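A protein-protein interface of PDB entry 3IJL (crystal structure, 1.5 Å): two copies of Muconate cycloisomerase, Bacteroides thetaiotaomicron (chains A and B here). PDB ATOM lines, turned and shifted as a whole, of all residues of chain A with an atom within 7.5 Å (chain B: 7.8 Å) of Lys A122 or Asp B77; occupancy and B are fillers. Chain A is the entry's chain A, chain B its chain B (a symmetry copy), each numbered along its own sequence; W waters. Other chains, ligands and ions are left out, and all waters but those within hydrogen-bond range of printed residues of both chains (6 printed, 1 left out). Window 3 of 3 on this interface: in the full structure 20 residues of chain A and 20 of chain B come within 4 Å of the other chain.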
ATOM      1  N   GLY A 117       3.126 -26.578   6.562  1.00  0.00           N
ATOM      2  CA  GLY A 117       3.271 -27.439   5.395  1.00  0.00           C
ATOM      3  C   GLY A 117       3.169 -26.767   4.042  1.00  0.00           C
ATOM      4  O   GLY A 117       2.776 -27.396   3.057  1.00  0.00           O
ATOM      5  N   LEU A 118       3.555 -25.499   3.980  1.00  0.00           N
ATOM      6  CA  LEU A 118       3.474 -24.732   2.743  1.00  0.00           C
ATOM      7  C   LEU A 118       4.783 -24.644   1.966  1.00  0.00           C
ATOM      8  O   LEU A 118       5.864 -24.814   2.525  1.00  0.00           O
ATOM      9  CB  LEU A 118       2.977 -23.321   3.059  1.00  0.00           C
ATOM     10  CG  LEU A 118       1.657 -23.295   3.830  1.00  0.00           C
ATOM     11  CD1 LEU A 118       1.298 -21.861   4.186  1.00  0.00           C
ATOM     12  CD2 LEU A 118       0.560 -23.940   2.994  1.00  0.00           C
ATOM     13  N   ASN A 119       4.659 -24.372   0.670  1.00  0.00           N
ATOM     14  CA  ASN A 119       5.806 -24.238  -0.225  1.00  0.00           C
ATOM     15  C   ASN A 119       6.146 -22.750  -0.306  1.00  0.00           C
ATOM     16  O   ASN A 119       5.382 -21.977  -0.873  1.00  0.00           O
ATOM     17  CB  ASN A 119       5.433 -24.754  -1.618  1.00  0.00           C
ATOM     18  CG  ASN A 119       6.618 -24.805  -2.563  1.00  0.00           C
ATOM     19  OD1 ASN A 119       7.550 -24.010  -2.455  1.00  0.00           O
ATOM     20  ND2 ASN A 119       6.578 -25.737  -3.509  1.00  0.00           N
ATOM     21  N   LYS A 120       7.285 -22.350   0.255  1.00  0.00           N
ATOM     22  CA  LYS A 120       7.673 -20.937   0.241  1.00  0.00           C
ATOM     23  C   LYS A 120       7.845 -20.374  -1.166  1.00  0.00           C
ATOM     24  O   LYS A 120       7.807 -19.159  -1.363  1.00  0.00           O
ATOM     25  CB  LYS A 120       8.966 -20.721   1.038  1.00  0.00           C
ATOM     26  CG  LYS A 120      10.208 -21.315   0.388  1.00  0.00           C
ATOM     27  CD  LYS A 120      11.456 -21.148   1.253  1.00  0.00           C
ATOM     28  CE  LYS A 120      11.921 -19.704   1.327  1.00  0.00           C
ATOM     29  NZ  LYS A 120      13.219 -19.581   2.058  1.00  0.00           N
ATOM     30  N   GLU A 121       8.038 -21.247  -2.151  1.00  0.00           N
ATOM     31  CA  GLU A 121       8.207 -20.771  -3.518  1.00  0.00           C
ATOM     32  C   GLU A 121       6.882 -20.314  -4.112  1.00  0.00           C
ATOM     33  O   GLU A 121       6.852 -19.716  -5.188  1.00  0.00           O
ATOM     34  CB  GLU A 121       8.828 -21.858  -4.399  1.00  0.00           C
ATOM     35  CG  GLU A 121      10.227 -22.271  -3.973  1.00  0.00           C
ATOM     36  CD  GLU A 121      11.139 -21.082  -3.722  1.00  0.00           C
ATOM     37  OE1 GLU A 121      11.184 -20.170  -4.574  1.00  0.00           O
ATOM     38  OE2 GLU A 121      11.819 -21.063  -2.674  1.00  0.00           O
ATOM     39  N   LYS A 122       5.787 -20.586  -3.407  1.00  0.00           N
ATOM     40  CA  LYS A 122       4.469 -20.187  -3.882  1.00  0.00           C
ATOM     41  C   LYS A 122       3.989 -18.867  -3.290  1.00  0.00           C
ATOM     42  O   LYS A 122       2.806 -18.530  -3.380  1.00  0.00           O
ATOM     43  CB  LYS A 122       3.449 -21.294  -3.612  1.00  0.00           C
ATOM     44  CG  LYS A 122       3.645 -22.514  -4.497  1.00  0.00           C
ATOM     45  CD  LYS A 122       2.568 -23.558  -4.248  1.00  0.00           C
ATOM     46  CE  LYS A 122       2.712 -24.730  -5.203  1.00  0.00           C
ATOM     47  NZ  LYS A 122       1.656 -25.749  -4.972  1.00  0.00           N
ATOM     48  N   THR A 123       4.902 -18.117  -2.683  1.00  0.00           N
ATOM     49  CA  THR A 123       4.538 -16.820  -2.127  1.00  0.00           C
ATOM     50  C   THR A 123       4.079 -15.941  -3.285  1.00  0.00           C
ATOM     51  O   THR A 123       4.508 -16.119  -4.423  1.00  0.00           O
ATOM     52  CB  THR A 123       5.724 -16.145  -1.426  1.00  0.00           C
ATOM     53  OG1 THR A 123       6.877 -16.221  -2.269  1.00  0.00           O
ATOM     54  CG2 THR A 123       6.013 -16.816  -0.083  1.00  0.00           C
ATOM     55  N   PRO A 124       3.197 -14.979  -3.008  1.00  0.00           N
ATOM     56  CA  PRO A 124       2.674 -14.080  -4.037  1.00  0.00           C
ATOM     57  C   PRO A 124       3.504 -12.834  -4.292  1.00  0.00           C
ATOM     58  O   PRO A 124       4.462 -12.539  -3.575  1.00  0.00           O
ATOM     59  CB  PRO A 124       1.313 -13.705  -3.475  1.00  0.00           C
ATOM     60  CG  PRO A 124       1.641 -13.540  -2.016  1.00  0.00           C
ATOM     61  CD  PRO A 124       2.493 -14.772  -1.729  1.00  0.00           C
ATOM     62  N   SER A 125       3.123 -12.117  -5.341  1.00  0.00           N
ATOM     63  CA  SER A 125       3.742 -10.845  -5.662  1.00  0.00           C
ATOM     64  C   SER A 125       2.946  -9.908  -4.772  1.00  0.00           C
ATOM     65  O   SER A 125       1.733 -10.077  -4.629  1.00  0.00           O
ATOM     66  CB  SER A 125       3.484 -10.444  -7.118  1.00  0.00           C
ATOM     67  OG  SER A 125       4.191 -11.260  -8.026  1.00  0.00           O
ATOM     68  N   PHE A 295       1.884 -17.323   5.876  1.00  0.00           N
ATOM     69  CA  PHE A 295       0.815 -18.095   5.241  1.00  0.00           C
ATOM     70  C   PHE A 295       0.491 -17.583   3.844  1.00  0.00           C
ATOM     71  O   PHE A 295      -0.466 -18.033   3.215  1.00  0.00           O
ATOM     72  CB  PHE A 295      -0.458 -18.140   6.116  1.00  0.00           C
ATOM     73  CG  PHE A 295      -1.078 -16.796   6.403  1.00  0.00           C
ATOM     74  CD1 PHE A 295      -1.899 -16.169   5.470  1.00  0.00           C
ATOM     75  CD2 PHE A 295      -0.863 -16.173   7.631  1.00  0.00           C
ATOM     76  CE1 PHE A 295      -2.499 -14.940   5.760  1.00  0.00           C
ATOM     77  CE2 PHE A 295      -1.457 -14.946   7.928  1.00  0.00           C
ATOM     78  CZ  PHE A 295      -2.275 -14.332   6.993  1.00  0.00           C
ATOM     79  N   SER A 296       1.307 -16.660   3.342  1.00  0.00           N
ATOM     80  CA  SER A 296       1.068 -16.103   2.014  1.00  0.00           C
ATOM     81  C   SER A 296       1.118 -17.131   0.877  1.00  0.00           C
ATOM     82  O   SER A 296       0.555 -16.895  -0.190  1.00  0.00           O
ATOM     83  CB  SER A 296       2.023 -14.930   1.728  1.00  0.00           C
ATOM     84  OG  SER A 296       3.378 -15.331   1.640  1.00  0.00           O
ATOM     85  N   PRO A 297       1.795 -18.280   1.074  1.00  0.00           N
ATOM     86  CA  PRO A 297       1.791 -19.223  -0.052  1.00  0.00           C
ATOM     87  C   PRO A 297       0.382 -19.736  -0.369  1.00  0.00           C
ATOM     88  O   PRO A 297       0.153 -20.329  -1.421  1.00  0.00           O
ATOM     89  CB  PRO A 297       2.707 -20.344   0.433  1.00  0.00           C
ATOM     90  CG  PRO A 297       3.710 -19.604   1.261  1.00  0.00           C
ATOM     91  CD  PRO A 297       2.840 -18.643   2.051  1.00  0.00           C
ATOM     92  N   ALA A 298      -0.558 -19.498   0.540  1.00  0.00           N
ATOM     93  CA  ALA A 298      -1.932 -19.957   0.353  1.00  0.00           C
ATOM     94  C   ALA A 298      -2.887 -18.882  -0.165  1.00  0.00           C
ATOM     95  O   ALA A 298      -4.078 -19.146  -0.345  1.00  0.00           O
ATOM     96  CB  ALA A 298      -2.461 -20.522   1.663  1.00  0.00           C
ATOM     97  N   VAL A 299      -2.380 -17.677  -0.410  1.00  0.00           N
ATOM     98  CA  VAL A 299      -3.236 -16.591  -0.879  1.00  0.00           C
ATOM     99  C   VAL A 299      -3.119 -16.302  -2.373  1.00  0.00           C
ATOM    100  O   VAL A 299      -2.126 -16.654  -3.013  1.00  0.00           O
ATOM    101  CB  VAL A 299      -2.954 -15.280  -0.103  1.00  0.00           C
ATOM    102  CG1 VAL A 299      -2.950 -15.556   1.394  1.00  0.00           C
ATOM    103  CG2 VAL A 299      -1.630 -14.675  -0.546  1.00  0.00           C
ATOM    104  N   LYS A 324       8.320 -10.309  -5.583  1.00  0.00           N
ATOM    105  CA  LYS A 324       7.732 -11.406  -4.826  1.00  0.00           C
ATOM    106  C   LYS A 324       8.063 -11.374  -3.334  1.00  0.00           C
ATOM    107  O   LYS A 324       9.193 -11.075  -2.952  1.00  0.00           O
ATOM    108  CB  LYS A 324       8.235 -12.712  -5.446  1.00  0.00           C
ATOM    109  CG  LYS A 324       7.413 -13.950  -5.205  1.00  0.00           C
ATOM    110  CD  LYS A 324       7.881 -15.027  -6.182  1.00  0.00           C
ATOM    111  CE  LYS A 324       7.079 -16.307  -6.060  1.00  0.00           C
ATOM    112  NZ  LYS A 324       7.298 -16.951  -4.746  1.00  0.00           N
ATOM    113  N   ILE A 325       7.072 -11.659  -2.493  1.00  0.00           N
ATOM    114  CA  ILE A 325       7.300 -11.718  -1.052  1.00  0.00           C
ATOM    115  C   ILE A 325       8.243 -12.898  -0.885  1.00  0.00           C
ATOM    116  O   ILE A 325       7.959 -13.999  -1.357  1.00  0.00           O
ATOM    117  CB  ILE A 325       5.985 -11.975  -0.284  1.00  0.00           C
ATOM    118  CG1 ILE A 325       5.163 -10.685  -0.238  1.00  0.00           C
ATOM    119  CG2 ILE A 325       6.284 -12.505   1.119  1.00  0.00           C
ATOM    120  CD1 ILE A 325       5.834  -9.543   0.499  1.00  0.00           C
ATOM    121  N   LEU A 327      10.320 -15.284   1.761  1.00  0.00           N
ATOM    122  CA  LEU A 327      10.540 -15.787   3.109  1.00  0.00           C
ATOM    123  C   LEU A 327      11.961 -16.306   3.281  1.00  0.00           C
ATOM    124  O   LEU A 327      12.491 -16.972   2.394  1.00  0.00           O
ATOM    125  CB  LEU A 327       9.566 -16.933   3.392  1.00  0.00           C
ATOM    126  CG  LEU A 327       8.090 -16.554   3.514  1.00  0.00           C
ATOM    127  CD1 LEU A 327       7.214 -17.780   3.283  1.00  0.00           C
ATOM    128  CD2 LEU A 327       7.841 -15.957   4.887  1.00  0.00           C
ATOM    129  N   PHE B  69       9.652 -35.827  -4.645  1.00  0.00           N
ATOM    130  CA  PHE B  69       9.556 -34.757  -3.654  1.00  0.00           C
ATOM    131  C   PHE B  69      10.778 -34.830  -2.746  1.00  0.00           C
ATOM    132  O   PHE B  69      11.048 -35.863  -2.140  1.00  0.00           O
ATOM    133  CB  PHE B  69       8.279 -34.914  -2.821  1.00  0.00           C
ATOM    134  CG  PHE B  69       7.018 -34.590  -3.573  1.00  0.00           C
ATOM    135  CD1 PHE B  69       6.626 -33.269  -3.769  1.00  0.00           C
ATOM    136  CD2 PHE B  69       6.227 -35.606  -4.093  1.00  0.00           C
ATOM    137  CE1 PHE B  69       5.460 -32.965  -4.471  1.00  0.00           C
ATOM    138  CE2 PHE B  69       5.060 -35.313  -4.798  1.00  0.00           C
ATOM    139  CZ  PHE B  69       4.675 -33.993  -4.986  1.00  0.00           C
ATOM    140  N   ASP B  71      11.327 -32.673  -0.125  1.00  0.00           N
ATOM    141  CA  ASP B  71      11.053 -32.085   1.182  1.00  0.00           C
ATOM    142  C   ASP B  71       9.733 -32.579   1.787  1.00  0.00           C
ATOM    143  O   ASP B  71       8.659 -32.177   1.351  1.00  0.00           O
ATOM    144  CB  ASP B  71      11.035 -30.565   1.008  1.00  0.00           C
ATOM    145  CG  ASP B  71      10.783 -29.818   2.295  1.00  0.00           C
ATOM    146  OD1 ASP B  71      10.687 -30.451   3.368  1.00  0.00           O
ATOM    147  OD2 ASP B  71      10.688 -28.576   2.216  1.00  0.00           O
ATOM    148  N   PHE B  73       8.228 -31.778   4.378  1.00  0.00           N
ATOM    149  CA  PHE B  73       7.438 -30.709   4.983  1.00  0.00           C
ATOM    150  C   PHE B  73       6.447 -30.052   4.029  1.00  0.00           C
ATOM    151  O   PHE B  73       5.609 -29.260   4.453  1.00  0.00           O
ATOM    152  CB  PHE B  73       8.367 -29.648   5.581  1.00  0.00           C
ATOM    153  CG  PHE B  73       8.983 -30.054   6.891  1.00  0.00           C
ATOM    154  CD1 PHE B  73       8.371 -29.720   8.095  1.00  0.00           C
ATOM    155  CD2 PHE B  73      10.164 -30.788   6.921  1.00  0.00           C
ATOM    156  CE1 PHE B  73       8.928 -30.112   9.316  1.00  0.00           C
ATOM    157  CE2 PHE B  73      10.727 -31.184   8.137  1.00  0.00           C
ATOM    158  CZ  PHE B  73      10.107 -30.845   9.333  1.00  0.00           C
ATOM    159  N   GLN B  74       6.547 -30.382   2.745  1.00  0.00           N
ATOM    160  CA  GLN B  74       5.644 -29.838   1.730  1.00  0.00           C
ATOM    161  C   GLN B  74       4.332 -30.615   1.767  1.00  0.00           C
ATOM    162  O   GLN B  74       3.884 -31.132   0.745  1.00  0.00           O
ATOM    163  CB  GLN B  74       6.264 -29.991   0.340  1.00  0.00           C
ATOM    164  CG  GLN B  74       7.577 -29.269   0.158  1.00  0.00           C
ATOM    165  CD  GLN B  74       7.431 -27.785   0.373  1.00  0.00           C
ATOM    166  OE1 GLN B  74       6.437 -27.187  -0.040  1.00  0.00           O
ATOM    167  NE2 GLN B  74       8.425 -27.174   1.007  1.00  0.00           N
ATOM    168  N   LEU B  75       3.710 -30.693   2.938  1.00  0.00           N
ATOM    169  CA  LEU B  75       2.472 -31.454   3.071  1.00  0.00           C
ATOM    170  C   LEU B  75       1.332 -30.983   2.175  1.00  0.00           C
ATOM    171  O   LEU B  75       0.579 -31.799   1.649  1.00  0.00           O
ATOM    172  CB  LEU B  75       2.018 -31.472   4.534  1.00  0.00           C
ATOM    173  CG  LEU B  75       2.987 -32.194   5.481  1.00  0.00           C
ATOM    174  CD1 LEU B  75       2.389 -32.262   6.879  1.00  0.00           C
ATOM    175  CD2 LEU B  75       3.270 -33.597   4.958  1.00  0.00           C
ATOM    176  N   GLU B  76       1.195 -29.675   1.999  1.00  0.00           N
ATOM    177  CA  GLU B  76       0.131 -29.155   1.151  1.00  0.00           C
ATOM    178  C   GLU B  76       0.299 -29.660  -0.282  1.00  0.00           C
ATOM    179  O   GLU B  76      -0.627 -30.223  -0.871  1.00  0.00           O
ATOM    180  CB  GLU B  76       0.150 -27.623   1.167  1.00  0.00           C
ATOM    181  CG  GLU B  76      -0.994 -26.968   0.398  1.00  0.00           C
ATOM    182  CD  GLU B  76      -2.363 -27.347   0.927  1.00  0.00           C
ATOM    183  OE1 GLU B  76      -2.520 -27.491   2.161  1.00  0.00           O
ATOM    184  OE2 GLU B  76      -3.298 -27.486   0.106  1.00  0.00           O
ATOM    185  N   ASP B  77       1.484 -29.459  -0.842  1.00  0.00           N
ATOM    186  CA  ASP B  77       1.755 -29.881  -2.210  1.00  0.00           C
ATOM    187  C   ASP B  77       1.718 -31.398  -2.377  1.00  0.00           C
ATOM    188  O   ASP B  77       1.098 -31.912  -3.309  1.00  0.00           O
ATOM    189  CB  ASP B  77       3.117 -29.354  -2.663  1.00  0.00           C
ATOM    190  CG  ASP B  77       3.106 -27.865  -2.958  1.00  0.00           C
ATOM    191  OD1 ASP B  77       2.089 -27.191  -2.688  1.00  0.00           O
ATOM    192  OD2 ASP B  77       4.131 -27.372  -3.465  1.00  0.00           O
ATOM    193  N   ILE B  78       2.378 -32.113  -1.472  1.00  0.00           N
ATOM    194  CA  ILE B  78       2.419 -33.568  -1.561  1.00  0.00           C
ATOM    195  C   ILE B  78       1.043 -34.216  -1.454  1.00  0.00           C
ATOM    196  O   ILE B  78       0.686 -35.063  -2.276  1.00  0.00           O
ATOM    197  CB  ILE B  78       3.327 -34.169  -0.466  1.00  0.00           C
ATOM    198  CG1 ILE B  78       4.774 -33.723  -0.688  1.00  0.00           C
ATOM    199  CG2 ILE B  78       3.247 -35.696  -0.496  1.00  0.00           C
ATOM    200  CD1 ILE B  78       5.689 -34.027   0.481  1.00  0.00           C
ATOM    201  N   LEU B  79       0.267 -33.828  -0.446  1.00  0.00           N
ATOM    202  CA  LEU B  79      -1.043 -34.431  -0.272  1.00  0.00           C
ATOM    203  C   LEU B  79      -2.056 -34.005  -1.329  1.00  0.00           C
ATOM    204  O   LEU B  79      -3.011 -34.734  -1.597  1.00  0.00           O
ATOM    205  CB  LEU B  79      -1.560 -34.175   1.146  1.00  0.00           C
ATOM    206  CG  LEU B  79      -0.705 -34.925   2.178  1.00  0.00           C
ATOM    207  CD1 LEU B  79      -1.151 -34.578   3.589  1.00  0.00           C
ATOM    208  CD2 LEU B  79      -0.815 -36.433   1.940  1.00  0.00           C
ATOM    209  N   SER B  80      -1.856 -32.837  -1.936  1.00  0.00           N
ATOM    210  CA  SER B  80      -2.756 -32.401  -3.001  1.00  0.00           C
ATOM    211  C   SER B  80      -2.463 -33.302  -4.199  1.00  0.00           C
ATOM    212  O   SER B  80      -3.372 -33.724  -4.918  1.00  0.00           O
ATOM    213  CB  SER B  80      -2.502 -30.940  -3.373  1.00  0.00           C
ATOM    214  OG  SER B  80      -2.918 -30.078  -2.327  1.00  0.00           O
ATOM    215  N   TYR B  81      -1.183 -33.592  -4.403  1.00  0.00           N
ATOM    216  CA  TYR B  81      -0.757 -34.468  -5.491  1.00  0.00           C
ATOM    217  C   TYR B  81      -1.328 -35.865  -5.264  1.00  0.00           C
ATOM    218  O   TYR B  81      -1.860 -36.487  -6.180  1.00  0.00           O
ATOM    219  CB  TYR B  81       0.773 -34.535  -5.546  1.00  0.00           C
ATOM    220  CG  TYR B  81       1.318 -35.803  -6.171  1.00  0.00           C
ATOM    221  CD1 TYR B  81       1.236 -36.024  -7.545  1.00  0.00           C
ATOM    222  CD2 TYR B  81       1.899 -36.790  -5.378  1.00  0.00           C
ATOM    223  CE1 TYR B  81       1.721 -37.205  -8.112  1.00  0.00           C
ATOM    224  CE2 TYR B  81       2.384 -37.967  -5.931  1.00  0.00           C
ATOM    225  CZ  TYR B  81       2.292 -38.168  -7.296  1.00  0.00           C
ATOM    226  OH  TYR B  81       2.779 -39.339  -7.826  1.00  0.00           O
ATOM    227  N   VAL B  82      -1.217 -36.358  -4.037  1.00  0.00           N
ATOM    228  CA  VAL B  82      -1.733 -37.683  -3.721  1.00  0.00           C
ATOM    229  C   VAL B  82      -3.243 -37.756  -3.977  1.00  0.00           C
ATOM    230  O   VAL B  82      -3.736 -38.721  -4.566  1.00  0.00           O
ATOM    231  CB  VAL B  82      -1.426 -38.053  -2.244  1.00  0.00           C
ATOM    232  CG1 VAL B  82      -2.195 -39.307  -1.838  1.00  0.00           C
ATOM    233  CG2 VAL B  82       0.073 -38.286  -2.076  1.00  0.00           C
ATOM    234  N   ASP B  83      -3.977 -36.733  -3.554  1.00  0.00           N
ATOM    235  CA  ASP B  83      -5.426 -36.725  -3.739  1.00  0.00           C
ATOM    236  C   ASP B  83      -5.804 -36.717  -5.223  1.00  0.00           C
ATOM    237  O   ASP B  83      -6.800 -37.322  -5.620  1.00  0.00           O
ATOM    238  CB  ASP B  83      -6.037 -35.511  -3.021  1.00  0.00           C
ATOM    239  CG  ASP B  83      -7.549 -35.612  -2.864  1.00  0.00           C
ATOM    240  OD1 ASP B  83      -8.074 -36.743  -2.792  1.00  0.00           O
ATOM    241  OD2 ASP B  83      -8.214 -34.553  -2.785  1.00  0.00           O
ATOM    242  N   SER B  84      -4.989 -36.057  -6.041  1.00  0.00           N
ATOM    243  CA  SER B  84      -5.256 -35.951  -7.476  1.00  0.00           C
ATOM    244  C   SER B  84      -5.140 -37.252  -8.267  1.00  0.00           C
ATOM    245  O   SER B  84      -5.654 -37.346  -9.383  1.00  0.00           O
ATOM    246  CB  SER B  84      -4.316 -34.921  -8.110  1.00  0.00           C
ATOM    247  OG  SER B  84      -3.013 -35.454  -8.279  1.00  0.00           O
ATOM    248  N   ARG B 261      -4.304 -34.245   7.905  1.00  0.00           N
ATOM    249  CA  ARG B 261      -4.367 -32.868   7.430  1.00  0.00           C
ATOM    250  C   ARG B 261      -5.802 -32.453   7.137  1.00  0.00           C
ATOM    251  O   ARG B 261      -6.242 -31.390   7.574  1.00  0.00           O
ATOM    252  CB  ARG B 261      -3.482 -32.668   6.194  1.00  0.00           C
ATOM    253  CG  ARG B 261      -3.268 -31.198   5.826  1.00  0.00           C
ATOM    254  CD  ARG B 261      -2.194 -31.055   4.757  1.00  0.00           C
ATOM    255  NE  ARG B 261      -1.954 -29.663   4.370  1.00  0.00           N
ATOM    256  CZ  ARG B 261      -1.160 -28.823   5.028  1.00  0.00           C
ATOM    257  NH1 ARG B 261      -0.515 -29.219   6.117  1.00  0.00           N
ATOM    258  NH2 ARG B 261      -0.999 -27.582   4.582  1.00  0.00           N
HETATM  259  O   HOH W   1       4.670 -29.527   7.527  1.00  0.00           O
HETATM  260  O   HOH W   2       1.537 -28.990   8.233  1.00  0.00           O
HETATM  261  O   HOH W   3       6.997 -26.675   4.126  1.00  0.00           O
HETATM  262  O   HOH W   4      -0.633 -27.318  -3.344  1.00  0.00           O
HETATM  263  O   HOH W   5       9.152 -24.533   0.897  1.00  0.00           O
HETATM  264  O   HOH W   6       2.101 -24.950  -0.661  1.00  0.00           O
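Water W3 lies within hydrogen-bond range of O of Leu A118 (2.7 Å), O of Phe B73 (3.0 Å) and NE2 of Gln B74 (3.5 Å). Water W5 lies within hydrogen-bond range of NE2 of Gln B74 and N of Lys A120. Water W4 bridges OD1 of Asp B77 (2.8 Å) and NZ of Lys A122 (3.2 Å). Water W6 lies within hydrogen-bond range of N of Asn A119 (2.9 Å) and OD1 of Asp B77 (3.0 Å). Water W2 bridges the guanidinium group of Arg B261 and the backbone NH of Gly A117. Water W1 lies within hydrogen-bond range of O of Phe B73 (3.2 Å) and N of Gly A117 (3.5 Å).
No position is printed for both chains. Of the 8 pairs that touch across the chains among the printed residues, none has its exchanged pair printed and touching as well.
The guanidinium group (NH2) of Arg B261 is in salt-bridge range of the side-chain carboxylate (OE1) of Glu B76, 2.9 Å away. N of Phe B73 is in hydrogen-bond range of OD1 of Asp B71 (3.0 Å). The backbone carbonyl oxygen of Glu B76 is in hydrogen-bond range of the side-chain hydroxyl of Ser B80, at 2.7 Å. OD2 of Asp B71 sits at hydrogen-bond distance from NE2 of Gln B74 (2.9 Å). The side-chain amide oxygen (OD1) of Asn A119 lies within hydrogen-bond range of the backbone NH (N) of Glu A121, at 2.8 Å.
The side-chain amide oxygen of Gln B74 sits close to the backbone NH of Asn A119 (3.4 Å). O of Gly A117 is in hydrogen-bond range of N of Glu B76 (3.0 Å). The side-chain amide nitrogen (ND2) of Asn A119 sits at hydrogen-bond distance from the side-chain carboxylate (OD2) of Asp B77 (2.9 Å). NZ of Lys A122 is in salt-bridge range of OD1 of Asp B77 (2.7 Å). O of Gly A117 is in hydrogen-bond range of N of Leu B75, at 3.4 Å.
Among the printed residues, 8 pairs touch across the chains. Among the printed residues, Asp or Glu carboxylates within 4 Å of a Lys or Arg side-chain nitrogen of the other chain: Lys A122 with Asp B77 (2.7 Å).
Among the printed residues, merely in contact across the chains: Gly A117 with Phe B73 (3.1 Å), Leu A118 with Gln B74 (3.5 Å) and Gly A117 with Gln B74 (3.8 Å).
Lys A122 touches just one residue of chain B: Asp B77 (2.7 Å). Asp B77 touches just these residues of chain A: Asn A119 (2.9 Å) and Lys A122 (2.7 Å). Of the printed residues of chain A, Leu B75 touches Gly A117. Printed residues of chain A within 4 Å of Phe B73: Gly A117 (3.1 Å). Of the printed residues of chain A, Glu B76 touches Gly A117 (3.0 Å). Of the printed residues of chain B, Leu A118 touches Gln B74 (3.5 Å). Of the printed residues of chain A, Gln B74 touches Gly A117 (3.8 Å), Leu A118 (3.5 Å) and Asn A119 (3.0 Å). Asp B71 touches none of the printed residues of chain A. Thr A123 touches none of the printed residues of chain B. The nearest residue of chain B that does not touch Lys A122 is Glu B76 (6.1 Å). The nearest printed residue of chain A that does not touch Phe B73 is Leu A118 (4.3 Å).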
